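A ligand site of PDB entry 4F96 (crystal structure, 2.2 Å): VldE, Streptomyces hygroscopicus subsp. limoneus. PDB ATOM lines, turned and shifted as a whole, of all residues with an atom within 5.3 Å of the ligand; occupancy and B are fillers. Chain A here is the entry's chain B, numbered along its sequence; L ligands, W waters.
The side-chain carboxylate (OE1) of Glu 391 is in hydrogen-bond range of an oxygen (O10) of the ligand, 2.5 Å away.
The side-chain amide oxygen (OD1) of Asn 361 is in hydrogen-bond range of a nitrogen (N3) of the ligand, at 2.6 Å.
N of Ser 388 lies within hydrogen-bond range of O6 of the ligand, 3.1 Å away.
An oxygen (O6) of the ligand sits at hydrogen-bond distance from the side-chain hydroxyl (OG) of Ser 388 (2.6 Å).
OG1 of Thr 366 is in hydrogen-bond range of N2 of the ligand.
An oxygen (O2) of the ligand is in salt-bridge range of the guanidinium group (NE) of Arg 290, at 2.8 Å.
The backbone NH (N) of Leu 387 is in hydrogen-bond range of an oxygen (O5) of the ligand.
The backbone NH of Asp 362 lies within hydrogen-bond range of an oxygen (O11) of the ligand (2.9 Å).
O1 of the ligand lies within salt-bridge range of NZ of Lys 295 (3.0 Å).
ND2 of Asn 323 lies close to N3 of the ligand (3.3 Å).
The guanidinium group (NH2) of Arg 321 sits at hydrogen-bond distance from an oxygen (O11) of the ligand, at 3.3 Å.
Water W4 lies within hydrogen-bond range of an oxygen (O11) of the ligand (2.7 Å), the backbone carbonyl oxygen of Asp 360 (3.2 Å), the side-chain hydroxyl of Thr 366 (3.2 Å), the backbone NH of Asn 323 (3.3 Å) and the guanidinium group of Arg 321 (3.3 Å).
Water W8 lies within hydrogen-bond range of an oxygen (O1) of the ligand and the guanidinium group (NH2) of Arg 290.
Water W9 bridges O5 of the ligand and N of Asn 386.
Water W2 lies within hydrogen-bond range of the side-chain amino group (NZ) of Lys 295 (2.8 Å), an oxygen (O6) of the ligand (2.8 Å) and the side-chain amide nitrogen (ND2) of Asn 386 (3.4 Å).
Water W3 bridges the backbone NH (N) of Arg 290 (2.7 Å) and an oxygen (O2) of the ligand (2.9 Å).
Water W7 lies within hydrogen-bond range of an oxygen (O8) of the ligand (2.9 Å) and the side-chain amide nitrogen of Asn 323 (3.0 Å).
O of Asp 360 sits close to O11 of the ligand (3.3 Å).
Merely in contact with the ligand: Asn 386 (3.3 Å) and Val 363 (3.7 Å).
Hydrophobic or aromatic side chains within 4 Å of the ligand: Val 363 and Leu 387.
13 residues have an atom within 4 Å of the ligand: Arg 290, Lys 295, Arg 321, Asn 323, Asp 360, Asn 361, Asp 362, Val 363, Thr 366, Asn 386, Leu 387, Ser 388 and Glu 391.
The nearest printed residue that does not touch the ligand is Asp 383 (4.02 Å).
The backbone NH (N) of Ser 388 lies within hydrogen-bond range of the side-chain amide oxygen (OD1) of Asn 386 (3.1 Å).
OG1 of Thr 366 sits at hydrogen-bond distance from NE of Arg 321 (2.8 Å).
The backbone carbonyl oxygen of Asp 362 is in hydrogen-bond range of the guanidinium group of Arg 321 (2.8 Å).
The side-chain amino group of Lys 295 lies within salt-bridge range of the side-chain carboxylate of Asp 383 (3.0 Å).
The guanidinium group (NH2) of Arg 321 is in hydrogen-bond range of the backbone carbonyl oxygen (O) of Asp 360.
ND2 of Asn 386 sits at hydrogen-bond distance from OD2 of Asp 383 (3.1 Å).
OD1 of Asn 386 lies within hydrogen-bond range of N of Thr 389 (2.8 Å).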
ATOM      1  N   SER A 288     -26.380  25.991 -11.001  1.00  0.00           N
ATOM      2  CA  SER A 288     -26.388  24.539 -10.972  1.00  0.00           C
ATOM      3  C   SER A 288     -26.732  23.962  -9.584  1.00  0.00           C
ATOM      4  O   SER A 288     -26.202  24.402  -8.560  1.00  0.00           O
ATOM      5  CB  SER A 288     -25.026  24.008 -11.425  1.00  0.00           C
ATOM      6  OG  SER A 288     -24.957  22.615 -11.284  1.00  0.00           O
ATOM      7  N   ARG A 290     -29.007  20.269  -7.641  1.00  0.00           N
ATOM      8  CA  ARG A 290     -30.021  19.243  -7.897  1.00  0.00           C
ATOM      9  C   ARG A 290     -31.459  19.776  -7.684  1.00  0.00           C
ATOM     10  O   ARG A 290     -31.655  20.941  -7.309  1.00  0.00           O
ATOM     11  CB  ARG A 290     -29.719  17.935  -7.144  1.00  0.00           C
ATOM     12  CG  ARG A 290     -29.909  17.987  -5.705  1.00  0.00           C
ATOM     13  CD  ARG A 290     -29.130  16.862  -4.939  1.00  0.00           C
ATOM     14  NE  ARG A 290     -28.808  17.481  -3.660  1.00  0.00           N
ATOM     15  CZ  ARG A 290     -29.729  17.785  -2.741  1.00  0.00           C
ATOM     16  NH1 ARG A 290     -31.004  17.441  -2.933  1.00  0.00           N
ATOM     17  NH2 ARG A 290     -29.374  18.397  -1.610  1.00  0.00           N
ATOM     18  N   ILE A 294     -33.997  23.950  -1.785  1.00  0.00           N
ATOM     19  CA  ILE A 294     -32.930  24.787  -1.220  1.00  0.00           C
ATOM     20  C   ILE A 294     -31.984  25.443  -2.258  1.00  0.00           C
ATOM     21  O   ILE A 294     -31.341  26.415  -1.959  1.00  0.00           O
ATOM     22  CB  ILE A 294     -32.040  24.019  -0.196  1.00  0.00           C
ATOM     23  CG1 ILE A 294     -31.221  22.924  -0.874  1.00  0.00           C
ATOM     24  CG2 ILE A 294     -32.903  23.450   0.944  1.00  0.00           C
ATOM     25  CD1 ILE A 294     -30.235  22.240   0.078  1.00  0.00           C
ATOM     26  N   LYS A 295     -31.880  24.887  -3.465  1.00  0.00           N
ATOM     27  CA  LYS A 295     -30.917  25.370  -4.433  1.00  0.00           C
ATOM     28  C   LYS A 295     -31.320  26.712  -5.030  1.00  0.00           C
ATOM     29  O   LYS A 295     -30.488  27.397  -5.640  1.00  0.00           O
ATOM     30  CB  LYS A 295     -30.725  24.327  -5.531  1.00  0.00           C
ATOM     31  CG  LYS A 295     -30.229  23.001  -5.017  1.00  0.00           C
ATOM     32  CD  LYS A 295     -28.906  23.194  -4.243  1.00  0.00           C
ATOM     33  CE  LYS A 295     -28.604  21.997  -3.365  1.00  0.00           C
ATOM     34  NZ  LYS A 295     -27.191  21.979  -2.877  1.00  0.00           N
ATOM     35  N   ARG A 321     -28.979  24.508 -14.686  1.00  0.00           N
ATOM     36  CA  ARG A 321     -28.581  23.136 -14.755  1.00  0.00           C
ATOM     37  C   ARG A 321     -29.064  22.472 -13.498  1.00  0.00           C
ATOM     38  O   ARG A 321     -28.722  22.918 -12.412  1.00  0.00           O
ATOM     39  CB  ARG A 321     -27.072  23.073 -14.834  1.00  0.00           C
ATOM     40  CG  ARG A 321     -26.520  21.698 -14.657  1.00  0.00           C
ATOM     41  CD  ARG A 321     -26.247  21.015 -15.971  1.00  0.00           C
ATOM     42  NE  ARG A 321     -25.720  19.673 -15.746  1.00  0.00           N
ATOM     43  CZ  ARG A 321     -26.145  18.593 -16.365  1.00  0.00           C
ATOM     44  NH1 ARG A 321     -27.115  18.697 -17.263  1.00  0.00           N
ATOM     45  NH2 ARG A 321     -25.614  17.406 -16.098  1.00  0.00           N
ATOM     46  N   ASN A 323     -29.882  18.571 -11.527  1.00  0.00           N
ATOM     47  CA  ASN A 323     -29.676  17.129 -11.446  1.00  0.00           C
ATOM     48  C   ASN A 323     -30.913  16.527 -10.767  1.00  0.00           C
ATOM     49  O   ASN A 323     -31.157  16.773  -9.594  1.00  0.00           O
ATOM     50  CB  ASN A 323     -28.388  16.802 -10.661  1.00  0.00           C
ATOM     51  CG  ASN A 323     -28.211  15.283 -10.393  1.00  0.00           C
ATOM     52  OD1 ASN A 323     -28.725  14.436 -11.132  1.00  0.00           O
ATOM     53  ND2 ASN A 323     -27.462  14.947  -9.329  1.00  0.00           N
ATOM     54  N   ASP A 360     -30.923  16.854 -15.815  1.00  0.00           N
ATOM     55  CA  ASP A 360     -30.185  15.715 -16.302  1.00  0.00           C
ATOM     56  C   ASP A 360     -29.082  15.320 -15.330  1.00  0.00           C
ATOM     57  O   ASP A 360     -28.440  16.164 -14.735  1.00  0.00           O
ATOM     58  CB  ASP A 360     -29.541  16.134 -17.639  1.00  0.00           C
ATOM     59  CG  ASP A 360     -29.260  14.992 -18.551  1.00  0.00           C
ATOM     60  OD1 ASP A 360     -28.704  15.218 -19.664  1.00  0.00           O
ATOM     61  OD2 ASP A 360     -29.634  13.880 -18.149  1.00  0.00           O
ATOM     62  N   ASN A 361     -28.859  14.027 -15.191  1.00  0.00           N
ATOM     63  CA  ASN A 361     -27.821  13.529 -14.323  1.00  0.00           C
ATOM     64  C   ASN A 361     -26.559  13.125 -15.099  1.00  0.00           C
ATOM     65  O   ASN A 361     -26.492  12.031 -15.671  1.00  0.00           O
ATOM     66  CB  ASN A 361     -28.347  12.365 -13.469  1.00  0.00           C
ATOM     67  CG  ASN A 361     -27.252  11.684 -12.685  1.00  0.00           C
ATOM     68  OD1 ASN A 361     -26.143  12.221 -12.500  1.00  0.00           O
ATOM     69  ND2 ASN A 361     -27.550  10.496 -12.189  1.00  0.00           N
ATOM     70  N   ASP A 362     -25.637  14.064 -15.239  1.00  0.00           N
ATOM     71  CA  ASP A 362     -24.336  13.801 -15.819  1.00  0.00           C
ATOM     72  C   ASP A 362     -23.334  14.709 -15.127  1.00  0.00           C
ATOM     73  O   ASP A 362     -23.333  15.906 -15.349  1.00  0.00           O
ATOM     74  CB  ASP A 362     -24.357  14.084 -17.316  1.00  0.00           C
ATOM     75  CG  ASP A 362     -23.215  13.414 -18.052  1.00  0.00           C
ATOM     76  OD1 ASP A 362     -23.460  12.900 -19.154  1.00  0.00           O
ATOM     77  OD2 ASP A 362     -22.086  13.418 -17.537  1.00  0.00           O
ATOM     78  N   VAL A 363     -22.458  14.137 -14.311  1.00  0.00           N
ATOM     79  CA  VAL A 363     -21.507  14.966 -13.597  1.00  0.00           C
ATOM     80  C   VAL A 363     -20.573  15.688 -14.577  1.00  0.00           C
ATOM     81  O   VAL A 363     -20.224  16.847 -14.370  1.00  0.00           O
ATOM     82  CB  VAL A 363     -20.721  14.187 -12.537  1.00  0.00           C
ATOM     83  CG1 VAL A 363     -19.674  13.294 -13.166  1.00  0.00           C
ATOM     84  CG2 VAL A 363     -20.091  15.144 -11.531  1.00  0.00           C
ATOM     85  N   THR A 366     -22.008  18.727 -16.053  1.00  0.00           N
ATOM     86  CA  THR A 366     -22.075  19.834 -15.095  1.00  0.00           C
ATOM     87  C   THR A 366     -20.736  20.540 -15.030  1.00  0.00           C
ATOM     88  O   THR A 366     -20.683  21.754 -15.063  1.00  0.00           O
ATOM     89  CB  THR A 366     -22.532  19.425 -13.691  1.00  0.00           C
ATOM     90  OG1 THR A 366     -23.903  19.026 -13.733  1.00  0.00           O
ATOM     91  CG2 THR A 366     -22.404  20.620 -12.717  1.00  0.00           C
ATOM     92  N   ILE A 367     -19.660  19.771 -14.990  1.00  0.00           N
ATOM     93  CA  ILE A 367     -18.324  20.337 -14.956  1.00  0.00           C
ATOM     94  C   ILE A 367     -18.035  21.167 -16.217  1.00  0.00           C
ATOM     95  O   ILE A 367     -17.390  22.216 -16.150  1.00  0.00           O
ATOM     96  CB  ILE A 367     -17.248  19.241 -14.773  1.00  0.00           C
ATOM     97  CG1 ILE A 367     -17.578  18.336 -13.559  1.00  0.00           C
ATOM     98  CG2 ILE A 367     -15.861  19.860 -14.685  1.00  0.00           C
ATOM     99  CD1 ILE A 367     -17.803  19.075 -12.273  1.00  0.00           C
ATOM    100  N   PHE A 370     -19.604  24.383 -15.684  1.00  0.00           N
ATOM    101  CA  PHE A 370     -18.736  25.185 -14.823  1.00  0.00           C
ATOM    102  C   PHE A 370     -17.628  25.847 -15.610  1.00  0.00           C
ATOM    103  O   PHE A 370     -17.340  27.023 -15.416  1.00  0.00           O
ATOM    104  CB  PHE A 370     -18.116  24.348 -13.685  1.00  0.00           C
ATOM    105  CG  PHE A 370     -19.122  23.883 -12.633  1.00  0.00           C
ATOM    106  CD1 PHE A 370     -20.398  24.400 -12.583  1.00  0.00           C
ATOM    107  CD2 PHE A 370     -18.749  22.938 -11.683  1.00  0.00           C
ATOM    108  CE1 PHE A 370     -21.305  23.979 -11.625  1.00  0.00           C
ATOM    109  CE2 PHE A 370     -19.654  22.500 -10.711  1.00  0.00           C
ATOM    110  CZ  PHE A 370     -20.933  23.029 -10.688  1.00  0.00           C
ATOM    111  N   ASP A 383     -27.654  26.008   2.667  1.00  0.00           N
ATOM    112  CA  ASP A 383     -26.954  24.793   2.247  1.00  0.00           C
ATOM    113  C   ASP A 383     -26.040  24.301   3.357  1.00  0.00           C
ATOM    114  O   ASP A 383     -25.416  25.104   4.035  1.00  0.00           O
ATOM    115  CB  ASP A 383     -26.148  25.052   0.974  1.00  0.00           C
ATOM    116  CG  ASP A 383     -26.451  24.051  -0.129  1.00  0.00           C
ATOM    117  OD1 ASP A 383     -26.598  22.856   0.170  1.00  0.00           O
ATOM    118  OD2 ASP A 383     -26.534  24.467  -1.297  1.00  0.00           O
ATOM    119  N   GLN A 385     -23.196  22.825   3.151  1.00  0.00           N
ATOM    120  CA  GLN A 385     -21.936  23.413   2.711  1.00  0.00           C
ATOM    121  C   GLN A 385     -22.062  23.976   1.301  1.00  0.00           C
ATOM    122  O   GLN A 385     -21.967  25.174   1.070  1.00  0.00           O
ATOM    123  CB  GLN A 385     -20.798  22.401   2.801  1.00  0.00           C
ATOM    124  CG  GLN A 385     -19.450  22.957   2.349  1.00  0.00           C
ATOM    125  CD  GLN A 385     -18.825  23.886   3.365  1.00  0.00           C
ATOM    126  OE1 GLN A 385     -19.499  24.428   4.235  1.00  0.00           O
ATOM    127  NE2 GLN A 385     -17.515  24.069   3.261  1.00  0.00           N
ATOM    128  N   ASN A 386     -22.257  23.058   0.362  1.00  0.00           N
ATOM    129  CA  ASN A 386     -22.242  23.361  -1.061  1.00  0.00           C
ATOM    130  C   ASN A 386     -20.793  23.256  -1.575  1.00  0.00           C
ATOM    131  O   ASN A 386     -19.997  24.202  -1.443  1.00  0.00           O
ATOM    132  CB  ASN A 386     -22.869  24.707  -1.444  1.00  0.00           C
ATOM    133  CG  ASN A 386     -23.064  24.865  -2.929  1.00  0.00           C
ATOM    134  OD1 ASN A 386     -22.079  24.877  -3.694  1.00  0.00           O
ATOM    135  ND2 ASN A 386     -24.344  24.994  -3.370  1.00  0.00           N
ATOM    136  N   LEU A 387     -20.488  22.090  -2.132  1.00  0.00           N
ATOM    137  CA  LEU A 387     -19.177  21.836  -2.739  1.00  0.00           C
ATOM    138  C   LEU A 387     -19.086  22.444  -4.147  1.00  0.00           C
ATOM    139  O   LEU A 387     -17.980  22.725  -4.622  1.00  0.00           O
ATOM    140  CB  LEU A 387     -18.887  20.344  -2.807  1.00  0.00           C
ATOM    141  CG  LEU A 387     -19.151  19.495  -1.555  1.00  0.00           C
ATOM    142  CD1 LEU A 387     -18.677  18.026  -1.786  1.00  0.00           C
ATOM    143  CD2 LEU A 387     -18.503  20.080  -0.315  1.00  0.00           C
ATOM    144  N   SER A 388     -20.228  22.606  -4.837  1.00  0.00           N
ATOM    145  CA  SER A 388     -20.202  23.101  -6.203  1.00  0.00           C
ATOM    146  C   SER A 388     -19.556  24.460  -6.234  1.00  0.00           C
ATOM    147  O   SER A 388     -18.903  24.817  -7.209  1.00  0.00           O
ATOM    148  CB  SER A 388     -21.594  23.210  -6.815  1.00  0.00           C
ATOM    149  OG  SER A 388     -22.275  21.967  -6.840  1.00  0.00           O
ATOM    150  N   THR A 389     -19.701  25.233  -5.166  1.00  0.00           N
ATOM    151  CA  THR A 389     -19.138  26.571  -5.181  1.00  0.00           C
ATOM    152  C   THR A 389     -17.606  26.576  -5.006  1.00  0.00           C
ATOM    153  O   THR A 389     -16.981  27.606  -5.232  1.00  0.00           O
ATOM    154  CB  THR A 389     -19.788  27.496  -4.112  1.00  0.00           C
ATOM    155  OG1 THR A 389     -19.324  28.838  -4.315  1.00  0.00           O
ATOM    156  CG2 THR A 389     -19.394  27.057  -2.754  1.00  0.00           C
ATOM    157  N   GLU A 391     -15.780  23.658  -6.415  1.00  0.00           N
ATOM    158  CA  GLU A 391     -15.473  23.017  -7.686  1.00  0.00           C
ATOM    159  C   GLU A 391     -15.489  24.008  -8.848  1.00  0.00           C
ATOM    160  O   GLU A 391     -14.558  24.029  -9.675  1.00  0.00           O
ATOM    161  CB  GLU A 391     -16.479  21.896  -7.990  1.00  0.00           C
ATOM    162  CG  GLU A 391     -16.449  20.725  -7.040  1.00  0.00           C
ATOM    163  CD  GLU A 391     -17.645  19.783  -7.225  1.00  0.00           C
ATOM    164  OE1 GLU A 391     -18.618  20.107  -7.970  1.00  0.00           O
ATOM    165  OE2 GLU A 391     -17.614  18.699  -6.594  1.00  0.00           O
HETATM  166  P1  LIG L   1     -25.553  18.770  -2.631  1.00  0.00           P
HETATM  167  O1  LIG L   1     -26.594  19.292  -1.684  1.00  0.00           O
HETATM  168  O2  LIG L   1     -26.105  18.154  -3.876  1.00  0.00           O
HETATM  169  O3  LIG L   1     -24.475  17.961  -1.965  1.00  0.00           O
HETATM  170  O4  LIG L   1     -24.820  20.079  -3.188  1.00  0.00           O
HETATM  171  P2  LIG L   1     -23.235  20.204  -3.420  1.00  0.00           P
HETATM  172  O5  LIG L   1     -22.555  20.190  -2.081  1.00  0.00           O
HETATM  173  O6  LIG L   1     -22.978  21.326  -4.381  1.00  0.00           O
HETATM  174  O7  LIG L   1     -22.868  18.826  -4.135  1.00  0.00           O
HETATM  175  C1  LIG L   1     -23.273  18.532  -5.457  1.00  0.00           C
HETATM  176  C2  LIG L   1     -22.296  17.534  -6.054  1.00  0.00           C
HETATM  177  O8  LIG L   1     -22.898  16.874  -7.154  1.00  0.00           O
HETATM  178  C3  LIG L   1     -21.062  18.239  -6.574  1.00  0.00           C
HETATM  179  O9  LIG L   1     -19.921  17.454  -6.281  1.00  0.00           O
HETATM  180  C4  LIG L   1     -21.283  18.289  -8.072  1.00  0.00           C
HETATM  181  O10 LIG L   1     -20.038  18.281  -8.782  1.00  0.00           O
HETATM  182  C5  LIG L   1     -22.088  17.023  -8.312  1.00  0.00           C
HETATM  183  N1  LIG L   1     -22.904  17.106  -9.538  1.00  0.00           N
HETATM  184  C6  LIG L   1     -23.110  18.183 -10.306  1.00  0.00           C
HETATM  185  N2  LIG L   1     -23.915  17.888 -11.347  1.00  0.00           N
HETATM  186  C7  LIG L   1     -24.229  16.592 -11.263  1.00  0.00           C
HETATM  187  C8  LIG L   1     -25.037  15.624 -12.043  1.00  0.00           C
HETATM  188  O11 LIG L   1     -25.639  15.987 -13.074  1.00  0.00           O
HETATM  189  N3  LIG L   1     -25.101  14.369 -11.602  1.00  0.00           N
HETATM  190  C9  LIG L   1     -24.461  13.950 -10.498  1.00  0.00           C
HETATM  191  N4  LIG L   1     -24.579  12.658 -10.126  1.00  0.00           N
HETATM  192  N5  LIG L   1     -23.707  14.778  -9.742  1.00  0.00           N
HETATM  193  C10 LIG L   1     -23.560  16.080 -10.073  1.00  0.00           C
HETATM  194  O   HOH W   1     -25.751  19.426  -8.609  1.00  0.00           O
HETATM  195  O   HOH W   2     -25.508  22.361  -5.112  1.00  0.00           O
HETATM  196  O   HOH W   3     -26.986  19.966  -5.939  1.00  0.00           O
HETATM  197  O   HOH W   4     -26.954  18.347 -12.986  1.00  0.00           O
HETATM  198  O   HOH W   5     -25.725  15.721  -4.912  1.00  0.00           O
HETATM  199  O   HOH W   6     -25.810  15.371  -0.441  1.00  0.00           O
HETATM  200  O   HOH W   7     -25.789  16.738  -7.545  1.00  0.00           O
HETATM  201  O   HOH W   8     -27.348  19.453   0.949  1.00  0.00           O
HETATM  202  O   HOH W   9     -22.423  20.153   0.687  1.00  0.00           O
